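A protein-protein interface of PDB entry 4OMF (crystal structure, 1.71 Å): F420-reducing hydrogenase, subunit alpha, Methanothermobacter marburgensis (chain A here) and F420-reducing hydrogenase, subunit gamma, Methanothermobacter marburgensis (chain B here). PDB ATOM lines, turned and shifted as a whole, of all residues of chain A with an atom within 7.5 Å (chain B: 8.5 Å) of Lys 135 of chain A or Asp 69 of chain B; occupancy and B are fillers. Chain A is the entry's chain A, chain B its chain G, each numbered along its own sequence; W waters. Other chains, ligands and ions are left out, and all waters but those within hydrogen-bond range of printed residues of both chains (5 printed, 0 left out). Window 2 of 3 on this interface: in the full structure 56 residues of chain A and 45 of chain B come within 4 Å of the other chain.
The side-chain carboxylate (OE1) of Glu 66 of chain B is in hydrogen-bond range of the side-chain hydroxyl (OH) of Tyr 68 of chain B, 2.5 Å away. The guanidinium group of Arg 134 of chain A sits at hydrogen-bond distance from the side-chain amide oxygen of Asn 104 of chain A (2.9 Å). The side-chain carboxylate of Glu 132 of chain A lies within salt-bridge range of the side-chain amino group of Lys 135 of chain A, 3.3 Å away.
Printed residues of chain B within 4 Å of Lys 135 of chain A: Tyr 68 (3.6 Å) and Asp 69 (2.8 Å). Of the printed residues of chain A, Asp 69 of chain B touches Lys 135 (2.8 Å). Of the printed residues of chain A, Leu 71 of chain B touches Ser 131. Printed residues of chain A within 4 Å of Glu 66 of chain B: Arg 134 (3.6 Å) and Gln 138 (3.1 Å). Tyr 139 of chain A touches none of the printed residues of chain B. Glu 132 of chain A touches none of the printed residues of chain B. The nearest residue of chain A that does not touch Asp 69 of chain B is Asn 128 of chain A (4.2 Å). The nearest printed residue of chain A that does not touch Tyr 68 of chain B is Arg 134 of chain A (4.01 Å).
The guanidinium group (NH1) of Arg 134 of chain A is in hydrogen-bond range of the side-chain hydroxyl (OG1) of Thr 65 of chain B (2.8 Å). The side-chain carboxylate (OE2) of Glu 66 of chain B sits at hydrogen-bond distance from the side-chain amide nitrogen (NE2) of Gln 138 of chain A, 3.1 Å away. The side-chain amino group (NZ) of Lys 135 of chain A lies within salt-bridge range of the side-chain carboxylate (OD1) of Asp 69 of chain B (2.8 Å).
Water W3 lies within hydrogen-bond range of the side-chain amide oxygen (OD1) of Asn 128 of chain A (2.5 Å), the backbone carbonyl oxygen (O) of Tyr 68 of chain B (2.8 Å) and the backbone NH (N) of Ala 72 of chain B (3.0 Å). Water W2 lies within hydrogen-bond range of OE2 of Glu 66 of chain B (2.7 Å), NH2 of Arg 134 of chain A (2.9 Å) and ND2 of Asn 104 of chain A (3.1 Å). Water W1 bridges OD1 of Asp 69 of chain B (2.8 Å) and OE1 of Glu 132 of chain A (2.9 Å). Water W5 lies within hydrogen-bond range of the side-chain hydroxyl (OH) of Tyr 68 of chain B (2.9 Å) and the backbone carbonyl oxygen (O) of Lys 135 of chain A (2.9 Å). Water W4 lies within hydrogen-bond range of the backbone carbonyl oxygen (O) of Thr 65 of chain B, the side-chain hydroxyl (OG) of Ser 131 of chain A and the guanidinium group (NH1) of Arg 134 of chain A.
Ala 72 of chain B touches Asn 128 of chain A. Ser 131 of chain A touches Tyr 68 of chain B (CB to O, 3.4 Å). Ser 131 of chain A touches Leu 71 of chain B. Arg 134 of chain A touches Glu 66 of chain B (NH2 to CG, 3.6 Å). Tyr 68 of chain B touches Lys 135 of chain A (CZ to CA, 3.6 Å). Gln 138 of chain A touches Tyr 68 of chain B (CB to OH, 3.6 Å).
Of the 19 printed residues of chain A, 5 touch a printed residue of chain B. Printed residues of chain A that touch a printed residue of chain B: Asn 128, Ser 131, Arg 134, Lys 135 and Gln 138. Of the 11 printed residues of chain B, 6 touch a printed residue of chain A. Printed residues of chain B that touch a printed residue of chain A: Thr 65, Glu 66, Tyr 68, Asp 69, Leu 71 and Ala 72. Hydrophobic or aromatic side chains of chain B within 4 Å of the printed part of chain A: Tyr 68, Leu 71 and Ala 72. Among the printed residues, Asp or Glu carboxylates within 4 Å of a Lys or Arg side-chain nitrogen of the other chain: Lys 135 of chain A with Asp 69 of chain B.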
ATOM      1  N   ASN A 104     -14.394  11.981  -3.579  1.00  0.00           N
ATOM      2  CA  ASN A 104     -15.801  11.599  -3.682  1.00  0.00           C
ATOM      3  C   ASN A 104     -16.728  12.819  -3.735  1.00  0.00           C
ATOM      4  O   ASN A 104     -17.574  12.935  -4.626  1.00  0.00           O
ATOM      5  CB  ASN A 104     -16.177  10.708  -2.501  1.00  0.00           C
ATOM      6  CG  ASN A 104     -17.601  10.176  -2.597  1.00  0.00           C
ATOM      7  OD1 ASN A 104     -18.062   9.797  -3.672  1.00  0.00           O
ATOM      8  ND2 ASN A 104     -18.297  10.135  -1.473  1.00  0.00           N
ATOM      9  N   ASN A 128     -20.816   8.455 -15.863  1.00  0.00           N
ATOM     10  CA  ASN A 128     -20.002   7.259 -15.704  1.00  0.00           C
ATOM     11  C   ASN A 128     -18.614   7.585 -15.174  1.00  0.00           C
ATOM     12  O   ASN A 128     -18.046   6.811 -14.403  1.00  0.00           O
ATOM     13  CB  ASN A 128     -19.900   6.497 -17.018  1.00  0.00           C
ATOM     14  CG  ASN A 128     -21.126   5.643 -17.275  1.00  0.00           C
ATOM     15  OD1 ASN A 128     -21.652   5.013 -16.347  1.00  0.00           O
ATOM     16  ND2 ASN A 128     -21.601   5.633 -18.509  1.00  0.00           N
ATOM     17  N   SER A 129     -18.075   8.733 -15.569  1.00  0.00           N
ATOM     18  CA  SER A 129     -16.767   9.161 -15.083  1.00  0.00           C
ATOM     19  C   SER A 129     -16.817   9.476 -13.592  1.00  0.00           C
ATOM     20  O   SER A 129     -15.966   9.035 -12.819  1.00  0.00           O
ATOM     21  CB  SER A 129     -16.275  10.385 -15.865  1.00  0.00           C
ATOM     22  OG  SER A 129     -15.070  10.904 -15.326  1.00  0.00           O
ATOM     23  N   VAL A 130     -17.812  10.270 -13.206  1.00  0.00           N
ATOM     24  CA  VAL A 130     -18.057  10.577 -11.815  1.00  0.00           C
ATOM     25  C   VAL A 130     -18.186   9.287 -11.030  1.00  0.00           C
ATOM     26  O   VAL A 130     -17.588   9.152  -9.950  1.00  0.00           O
ATOM     27  CB  VAL A 130     -19.326  11.433 -11.640  1.00  0.00           C
ATOM     28  CG1 VAL A 130     -19.803  11.376 -10.200  1.00  0.00           C
ATOM     29  CG2 VAL A 130     -19.038  12.881 -12.063  1.00  0.00           C
ATOM     30  N   SER A 131     -18.959   8.343 -11.554  1.00  0.00           N
ATOM     31  CA  SER A 131     -19.256   7.131 -10.790  1.00  0.00           C
ATOM     32  C   SER A 131     -18.014   6.250 -10.582  1.00  0.00           C
ATOM     33  O   SER A 131     -17.823   5.680  -9.507  1.00  0.00           O
ATOM     34  CB  SER A 131     -20.378   6.322 -11.476  1.00  0.00           C
ATOM     35  OG  SER A 131     -21.577   7.094 -11.469  1.00  0.00           O
ATOM     36  N   GLU A 132     -17.162   6.142 -11.594  1.00  0.00           N
ATOM     37  CA  GLU A 132     -15.968   5.316 -11.424  1.00  0.00           C
ATOM     38  C   GLU A 132     -15.019   5.967 -10.418  1.00  0.00           C
ATOM     39  O   GLU A 132     -14.346   5.277  -9.629  1.00  0.00           O
ATOM     40  CB  GLU A 132     -15.250   5.075 -12.764  1.00  0.00           C
ATOM     41  CG  GLU A 132     -14.064   4.095 -12.664  1.00  0.00           C
ATOM     42  CD  GLU A 132     -14.474   2.664 -12.233  1.00  0.00           C
ATOM     43  OE1 GLU A 132     -15.658   2.268 -12.426  1.00  0.00           O
ATOM     44  OE2 GLU A 132     -13.599   1.937 -11.689  1.00  0.00           O
ATOM     45  N   ILE A 133     -14.970   7.291 -10.436  1.00  0.00           N
ATOM     46  CA  ILE A 133     -14.107   7.996  -9.507  1.00  0.00           C
ATOM     47  C   ILE A 133     -14.620   7.789  -8.073  1.00  0.00           C
ATOM     48  O   ILE A 133     -13.854   7.487  -7.149  1.00  0.00           O
ATOM     49  CB  ILE A 133     -14.050   9.493  -9.869  1.00  0.00           C
ATOM     50  CG1 ILE A 133     -13.191   9.655 -11.130  1.00  0.00           C
ATOM     51  CG2 ILE A 133     -13.507  10.297  -8.724  1.00  0.00           C
ATOM     52  CD1 ILE A 133     -13.191  11.103 -11.724  1.00  0.00           C
ATOM     53  N   ARG A 134     -15.927   7.945  -7.881  1.00  0.00           N
ATOM     54  CA  ARG A 134     -16.501   7.772  -6.544  1.00  0.00           C
ATOM     55  C   ARG A 134     -16.335   6.338  -6.046  1.00  0.00           C
ATOM     56  O   ARG A 134     -16.083   6.125  -4.854  1.00  0.00           O
ATOM     57  CB  ARG A 134     -17.981   8.134  -6.546  1.00  0.00           C
ATOM     58  CG  ARG A 134     -18.213   9.601  -6.803  1.00  0.00           C
ATOM     59  CD  ARG A 134     -19.716   9.847  -6.836  1.00  0.00           C
ATOM     60  NE  ARG A 134     -20.290   9.680  -5.504  1.00  0.00           N
ATOM     61  CZ  ARG A 134     -21.601   9.589  -5.257  1.00  0.00           C
ATOM     62  NH1 ARG A 134     -22.479   9.654  -6.249  1.00  0.00           N
ATOM     63  NH2 ARG A 134     -22.035   9.466  -4.005  1.00  0.00           N
ATOM     64  N   LYS A 135     -16.515   5.363  -6.944  1.00  0.00           N
ATOM     65  CA  LYS A 135     -16.353   3.956  -6.563  1.00  0.00           C
ATOM     66  C   LYS A 135     -14.982   3.727  -5.926  1.00  0.00           C
ATOM     67  O   LYS A 135     -14.867   3.109  -4.876  1.00  0.00           O
ATOM     68  CB  LYS A 135     -16.506   3.033  -7.760  1.00  0.00           C
ATOM     69  CG  LYS A 135     -16.302   1.537  -7.412  1.00  0.00           C
ATOM     70  CD  LYS A 135     -16.160   0.652  -8.650  1.00  0.00           C
ATOM     71  CE  LYS A 135     -17.369   0.679  -9.550  1.00  0.00           C
ATOM     72  NZ  LYS A 135     -17.152  -0.202 -10.759  1.00  0.00           N
ATOM     73  N   ASN A 136     -13.941   4.237  -6.565  1.00  0.00           N
ATOM     74  CA  ASN A 136     -12.592   4.007  -6.053  1.00  0.00           C
ATOM     75  C   ASN A 136     -12.254   4.802  -4.795  1.00  0.00           C
ATOM     76  O   ASN A 136     -11.631   4.279  -3.858  1.00  0.00           O
ATOM     77  CB  ASN A 136     -11.601   4.297  -7.185  1.00  0.00           C
ATOM     78  CG  ASN A 136     -11.553   3.159  -8.180  1.00  0.00           C
ATOM     79  OD1 ASN A 136     -10.787   2.218  -7.992  1.00  0.00           O
ATOM     80  ND2 ASN A 136     -12.399   3.212  -9.222  1.00  0.00           N
ATOM     81  N   ALA A 137     -12.663   6.065  -4.764  1.00  0.00           N
ATOM     82  CA  ALA A 137     -12.542   6.860  -3.552  1.00  0.00           C
ATOM     83  C   ALA A 137     -13.239   6.171  -2.370  1.00  0.00           C
ATOM     84  O   ALA A 137     -12.713   6.105  -1.264  1.00  0.00           O
ATOM     85  CB  ALA A 137     -13.121   8.259  -3.778  1.00  0.00           C
ATOM     86  N   GLN A 138     -14.433   5.657  -2.607  1.00  0.00           N
ATOM     87  CA  GLN A 138     -15.188   5.080  -1.508  1.00  0.00           C
ATOM     88  C   GLN A 138     -14.666   3.714  -1.020  1.00  0.00           C
ATOM     89  O   GLN A 138     -14.957   3.329   0.119  1.00  0.00           O
ATOM     90  CB  GLN A 138     -16.667   4.991  -1.903  1.00  0.00           C
ATOM     91  CG  GLN A 138     -17.367   6.382  -1.930  1.00  0.00           C
ATOM     92  CD  GLN A 138     -17.528   6.966  -0.543  1.00  0.00           C
ATOM     93  OE1 GLN A 138     -16.567   7.454   0.063  1.00  0.00           O
ATOM     94  NE2 GLN A 138     -18.746   6.894  -0.015  1.00  0.00           N
ATOM     95  N   TYR A 139     -13.889   2.985  -1.830  1.00  0.00           N
ATOM     96  CA  TYR A 139     -13.184   1.821  -1.271  1.00  0.00           C
ATOM     97  C   TYR A 139     -12.390   2.221  -0.033  1.00  0.00           C
ATOM     98  O   TYR A 139     -12.320   1.473   0.945  1.00  0.00           O
ATOM     99  CB  TYR A 139     -12.214   1.205  -2.262  1.00  0.00           C
ATOM    100  CG  TYR A 139     -12.814   0.493  -3.458  1.00  0.00           C
ATOM    101  CD1 TYR A 139     -13.857  -0.425  -3.312  1.00  0.00           C
ATOM    102  CD2 TYR A 139     -12.312   0.724  -4.731  1.00  0.00           C
ATOM    103  CE1 TYR A 139     -14.381  -1.092  -4.422  1.00  0.00           C
ATOM    104  CE2 TYR A 139     -12.828   0.089  -5.829  1.00  0.00           C
ATOM    105  CZ  TYR A 139     -13.870  -0.814  -5.682  1.00  0.00           C
ATOM    106  OH  TYR A 139     -14.357  -1.458  -6.797  1.00  0.00           O
ATOM    107  N   VAL A 140     -11.737   3.370  -0.103  1.00  0.00           N
ATOM    108  CA  VAL A 140     -10.936   3.842   1.037  1.00  0.00           C
ATOM    109  C   VAL A 140     -11.789   4.127   2.269  1.00  0.00           C
ATOM    110  O   VAL A 140     -11.488   3.671   3.396  1.00  0.00           O
ATOM    111  CB  VAL A 140     -10.148   5.126   0.683  1.00  0.00           C
ATOM    112  CG1 VAL A 140      -9.332   5.586   1.887  1.00  0.00           C
ATOM    113  CG2 VAL A 140      -9.197   4.892  -0.493  1.00  0.00           C
ATOM    114  N   VAL A 141     -12.847   4.898   2.069  1.00  0.00           N
ATOM    115  CA  VAL A 141     -13.670   5.294   3.205  1.00  0.00           C
ATOM    116  C   VAL A 141     -14.354   4.076   3.851  1.00  0.00           C
ATOM    117  O   VAL A 141     -14.368   3.980   5.071  1.00  0.00           O
ATOM    118  CB  VAL A 141     -14.728   6.330   2.820  1.00  0.00           C
ATOM    119  CG1 VAL A 141     -15.499   6.768   4.062  1.00  0.00           C
ATOM    120  CG2 VAL A 141     -14.051   7.570   2.148  1.00  0.00           C
ATOM    121  N   ASP A 142     -14.895   3.155   3.047  1.00  0.00           N
ATOM    122  CA  ASP A 142     -15.451   1.896   3.584  1.00  0.00           C
ATOM    123  C   ASP A 142     -14.387   1.070   4.351  1.00  0.00           C
ATOM    124  O   ASP A 142     -14.599   0.710   5.522  1.00  0.00           O
ATOM    125  CB  ASP A 142     -16.046   1.019   2.471  1.00  0.00           C
ATOM    126  CG  ASP A 142     -17.503   1.369   2.124  1.00  0.00           C
ATOM    127  OD1 ASP A 142     -18.366   1.468   3.038  1.00  0.00           O
ATOM    128  OD2 ASP A 142     -17.776   1.540   0.911  1.00  0.00           O
ATOM    129  N   ARG A 174      -5.382   0.861  -6.460  1.00  0.00           N
ATOM    130  CA  ARG A 174      -6.571   1.405  -7.114  1.00  0.00           C
ATOM    131  C   ARG A 174      -6.521   2.937  -7.217  1.00  0.00           C
ATOM    132  O   ARG A 174      -6.849   3.486  -8.268  1.00  0.00           O
ATOM    133  CB  ARG A 174      -7.833   0.933  -6.400  1.00  0.00           C
ATOM    134  CG  ARG A 174      -8.075  -0.547  -6.708  1.00  0.00           C
ATOM    135  CD  ARG A 174      -9.288  -1.077  -5.992  1.00  0.00           C
ATOM    136  NE  ARG A 174      -9.390  -2.525  -6.159  1.00  0.00           N
ATOM    137  CZ  ARG A 174     -10.259  -3.283  -5.492  1.00  0.00           C
ATOM    138  NH1 ARG A 174     -11.113  -2.721  -4.629  1.00  0.00           N
ATOM    139  NH2 ARG A 174     -10.268  -4.600  -5.679  1.00  0.00           N
ATOM    140  N   LEU A 175      -6.070   3.605  -6.159  1.00  0.00           N
ATOM    141  CA  LEU A 175      -5.940   5.062  -6.196  1.00  0.00           C
ATOM    142  C   LEU A 175      -4.846   5.498  -7.170  1.00  0.00           C
ATOM    143  O   LEU A 175      -5.036   6.452  -7.921  1.00  0.00           O
ATOM    144  CB  LEU A 175      -5.657   5.635  -4.789  1.00  0.00           C
ATOM    145  CG  LEU A 175      -6.794   5.543  -3.765  1.00  0.00           C
ATOM    146  CD1 LEU A 175      -6.506   6.518  -2.635  1.00  0.00           C
ATOM    147  CD2 LEU A 175      -8.143   5.862  -4.370  1.00  0.00           C
ATOM    148  N   LEU A 178      -6.004   5.280 -10.581  1.00  0.00           N
ATOM    149  CA  LEU A 178      -7.079   6.265 -10.752  1.00  0.00           C
ATOM    150  C   LEU A 178      -6.522   7.637 -11.149  1.00  0.00           C
ATOM    151  O   LEU A 178      -7.264   8.480 -11.668  1.00  0.00           O
ATOM    152  CB  LEU A 178      -7.913   6.417  -9.453  1.00  0.00           C
ATOM    153  CG  LEU A 178      -9.223   7.218  -9.592  1.00  0.00           C
ATOM    154  CD1 LEU A 178     -10.213   6.416 -10.415  1.00  0.00           C
ATOM    155  CD2 LEU A 178      -9.815   7.598  -8.247  1.00  0.00           C
ATOM    156  N   LEU B  64     -28.224   5.800  -3.053  1.00  0.00           N
ATOM    157  CA  LEU B  64     -28.828   5.452  -4.333  1.00  0.00           C
ATOM    158  C   LEU B  64     -27.788   5.670  -5.433  1.00  0.00           C
ATOM    159  O   LEU B  64     -27.624   4.831  -6.330  1.00  0.00           O
ATOM    160  CB  LEU B  64     -30.090   6.293  -4.600  1.00  0.00           C
ATOM    161  CG  LEU B  64     -30.749   6.102  -5.986  1.00  0.00           C
ATOM    162  CD1 LEU B  64     -32.245   6.344  -5.917  1.00  0.00           C
ATOM    163  CD2 LEU B  64     -30.135   7.029  -7.022  1.00  0.00           C
ATOM    164  N   THR B  65     -27.060   6.788  -5.355  1.00  0.00           N
ATOM    165  CA  THR B  65     -26.157   7.124  -6.451  1.00  0.00           C
ATOM    166  C   THR B  65     -24.856   6.321  -6.389  1.00  0.00           C
ATOM    167  O   THR B  65     -24.053   6.398  -7.301  1.00  0.00           O
ATOM    168  CB  THR B  65     -25.788   8.638  -6.492  1.00  0.00           C
ATOM    169  OG1 THR B  65     -25.081   9.018  -5.299  1.00  0.00           O
ATOM    170  CG2 THR B  65     -27.042   9.528  -6.696  1.00  0.00           C
ATOM    171  N   GLU B  66     -24.648   5.537  -5.330  1.00  0.00           N
ATOM    172  CA  GLU B  66     -23.466   4.695  -5.272  1.00  0.00           C
ATOM    173  C   GLU B  66     -23.731   3.305  -5.879  1.00  0.00           C
ATOM    174  O   GLU B  66     -22.948   2.383  -5.691  1.00  0.00           O
ATOM    175  CB  GLU B  66     -22.951   4.601  -3.823  1.00  0.00           C
ATOM    176  CG  GLU B  66     -22.287   5.933  -3.418  1.00  0.00           C
ATOM    177  CD  GLU B  66     -21.309   5.782  -2.227  1.00  0.00           C
ATOM    178  OE1 GLU B  66     -20.303   5.075  -2.376  1.00  0.00           O
ATOM    179  OE2 GLU B  66     -21.561   6.383  -1.172  1.00  0.00           O
ATOM    180  N   ASN B  67     -24.832   3.174  -6.624  1.00  0.00           N
ATOM    181  CA  ASN B  67     -24.963   2.126  -7.623  1.00  0.00           C
ATOM    182  C   ASN B  67     -24.198   2.559  -8.862  1.00  0.00           C
ATOM    183  O   ASN B  67     -24.792   2.967  -9.855  1.00  0.00           O
ATOM    184  CB  ASN B  67     -26.439   1.866  -7.926  1.00  0.00           C
ATOM    185  CG  ASN B  67     -27.106   1.132  -6.803  1.00  0.00           C
ATOM    186  OD1 ASN B  67     -26.799  -0.033  -6.581  1.00  0.00           O
ATOM    187  ND2 ASN B  67     -27.978   1.807  -6.049  1.00  0.00           N
ATOM    188  N   TYR B  68     -22.866   2.501  -8.772  1.00  0.00           N
ATOM    189  CA  TYR B  68     -22.011   3.228  -9.703  1.00  0.00           C
ATOM    190  C   TYR B  68     -22.199   2.812 -11.149  1.00  0.00           C
ATOM    191  O   TYR B  68     -22.376   3.654 -12.029  1.00  0.00           O
ATOM    192  CB  TYR B  68     -20.536   3.046  -9.348  1.00  0.00           C
ATOM    193  CG  TYR B  68     -20.217   3.146  -7.881  1.00  0.00           C
ATOM    194  CD1 TYR B  68     -19.914   2.002  -7.150  1.00  0.00           C
ATOM    195  CD2 TYR B  68     -20.183   4.387  -7.227  1.00  0.00           C
ATOM    196  CE1 TYR B  68     -19.597   2.059  -5.807  1.00  0.00           C
ATOM    197  CE2 TYR B  68     -19.874   4.454  -5.876  1.00  0.00           C
ATOM    198  CZ  TYR B  68     -19.584   3.276  -5.174  1.00  0.00           C
ATOM    199  OH  TYR B  68     -19.257   3.305  -3.829  1.00  0.00           O
ATOM    200  N   ASP B  69     -22.144   1.504 -11.396  1.00  0.00           N
ATOM    201  CA  ASP B  69     -22.096   1.020 -12.761  1.00  0.00           C
ATOM    202  C   ASP B  69     -23.386   1.289 -13.515  1.00  0.00           C
ATOM    203  O   ASP B  69     -23.365   1.589 -14.725  1.00  0.00           O
ATOM    204  CB  ASP B  69     -21.798  -0.475 -12.793  1.00  0.00           C
ATOM    205  CG  ASP B  69     -20.376  -0.790 -12.376  1.00  0.00           C
ATOM    206  OD1 ASP B  69     -19.581   0.159 -12.149  1.00  0.00           O
ATOM    207  OD2 ASP B  69     -20.057  -1.993 -12.289  1.00  0.00           O
ATOM    208  N   ILE B  70     -24.511   1.223 -12.810  1.00  0.00           N
ATOM    209  CA  ILE B  70     -25.794   1.345 -13.494  1.00  0.00           C
ATOM    210  C   ILE B  70     -26.389   2.745 -13.461  1.00  0.00           C
ATOM    211  O   ILE B  70     -27.365   3.010 -14.147  1.00  0.00           O
ATOM    212  CB  ILE B  70     -26.838   0.382 -12.914  1.00  0.00           C
ATOM    213  CG1 ILE B  70     -27.277   0.821 -11.516  1.00  0.00           C
ATOM    214  CG2 ILE B  70     -26.317  -1.041 -12.953  1.00  0.00           C
ATOM    215  CD1 ILE B  70     -28.440   0.024 -10.983  1.00  0.00           C
ATOM    216  N   LEU B  71     -25.784   3.646 -12.699  1.00  0.00           N
ATOM    217  CA  LEU B  71     -26.420   4.948 -12.434  1.00  0.00           C
ATOM    218  C   LEU B  71     -26.813   5.719 -13.689  1.00  0.00           C
ATOM    219  O   LEU B  71     -27.942   6.224 -13.781  1.00  0.00           O
ATOM    220  CB  LEU B  71     -25.518   5.818 -11.554  1.00  0.00           C
ATOM    221  CG  LEU B  71     -26.191   7.130 -11.131  1.00  0.00           C
ATOM    222  CD1 LEU B  71     -27.416   6.823 -10.261  1.00  0.00           C
ATOM    223  CD2 LEU B  71     -25.203   8.087 -10.406  1.00  0.00           C
ATOM    224  N   ALA B  72     -25.916   5.800 -14.668  1.00  0.00           N
ATOM    225  CA  ALA B  72     -26.232   6.564 -15.870  1.00  0.00           C
ATOM    226  C   ALA B  72     -27.460   5.953 -16.570  1.00  0.00           C
ATOM    227  O   ALA B  72     -28.392   6.670 -16.928  1.00  0.00           O
ATOM    228  CB  ALA B  72     -25.033   6.623 -16.813  1.00  0.00           C
ATOM    229  N   GLU B  73     -27.476   4.633 -16.701  1.00  0.00           N
ATOM    230  CA  GLU B  73     -28.578   3.928 -17.359  1.00  0.00           C
ATOM    231  C   GLU B  73     -29.877   4.031 -16.540  1.00  0.00           C
ATOM    232  O   GLU B  73     -30.982   4.166 -17.097  1.00  0.00           O
ATOM    233  CB  GLU B  73     -28.187   2.460 -17.590  1.00  0.00           C
ATOM    234  CG  GLU B  73     -29.217   1.611 -18.309  1.00  0.00           C
ATOM    235  CD  GLU B  73     -29.346   1.952 -19.790  1.00  0.00           C
ATOM    236  OE1 GLU B  73     -28.476   2.672 -20.332  1.00  0.00           O
ATOM    237  OE2 GLU B  73     -30.329   1.493 -20.409  1.00  0.00           O
ATOM    238  N   LEU B  74     -29.736   3.956 -15.222  1.00  0.00           N
ATOM    239  CA  LEU B  74     -30.872   4.098 -14.315  1.00  0.00           C
ATOM    240  C   LEU B  74     -31.586   5.435 -14.517  1.00  0.00           C
ATOM    241  O   LEU B  74     -32.793   5.471 -14.777  1.00  0.00           O
ATOM    242  CB  LEU B  74     -30.409   3.960 -12.853  1.00  0.00           C
ATOM    243  CG  LEU B  74     -31.454   4.213 -11.761  1.00  0.00           C
ATOM    244  CD1 LEU B  74     -32.554   3.176 -11.855  1.00  0.00           C
ATOM    245  CD2 LEU B  74     -30.811   4.192 -10.357  1.00  0.00           C
HETATM  246  O   HOH W   1     -18.502   2.781 -12.382  1.00  0.00           O
HETATM  247  O   HOH W   2     -21.233   9.037  -1.247  1.00  0.00           O
HETATM  248  O   HOH W   3     -23.007   5.143 -14.278  1.00  0.00           O
HETATM  249  O   HOH W   4     -22.005   7.860  -8.672  1.00  0.00           O
HETATM  250  O   HOH W   5     -16.956   1.649  -3.514  1.00  0.00           O
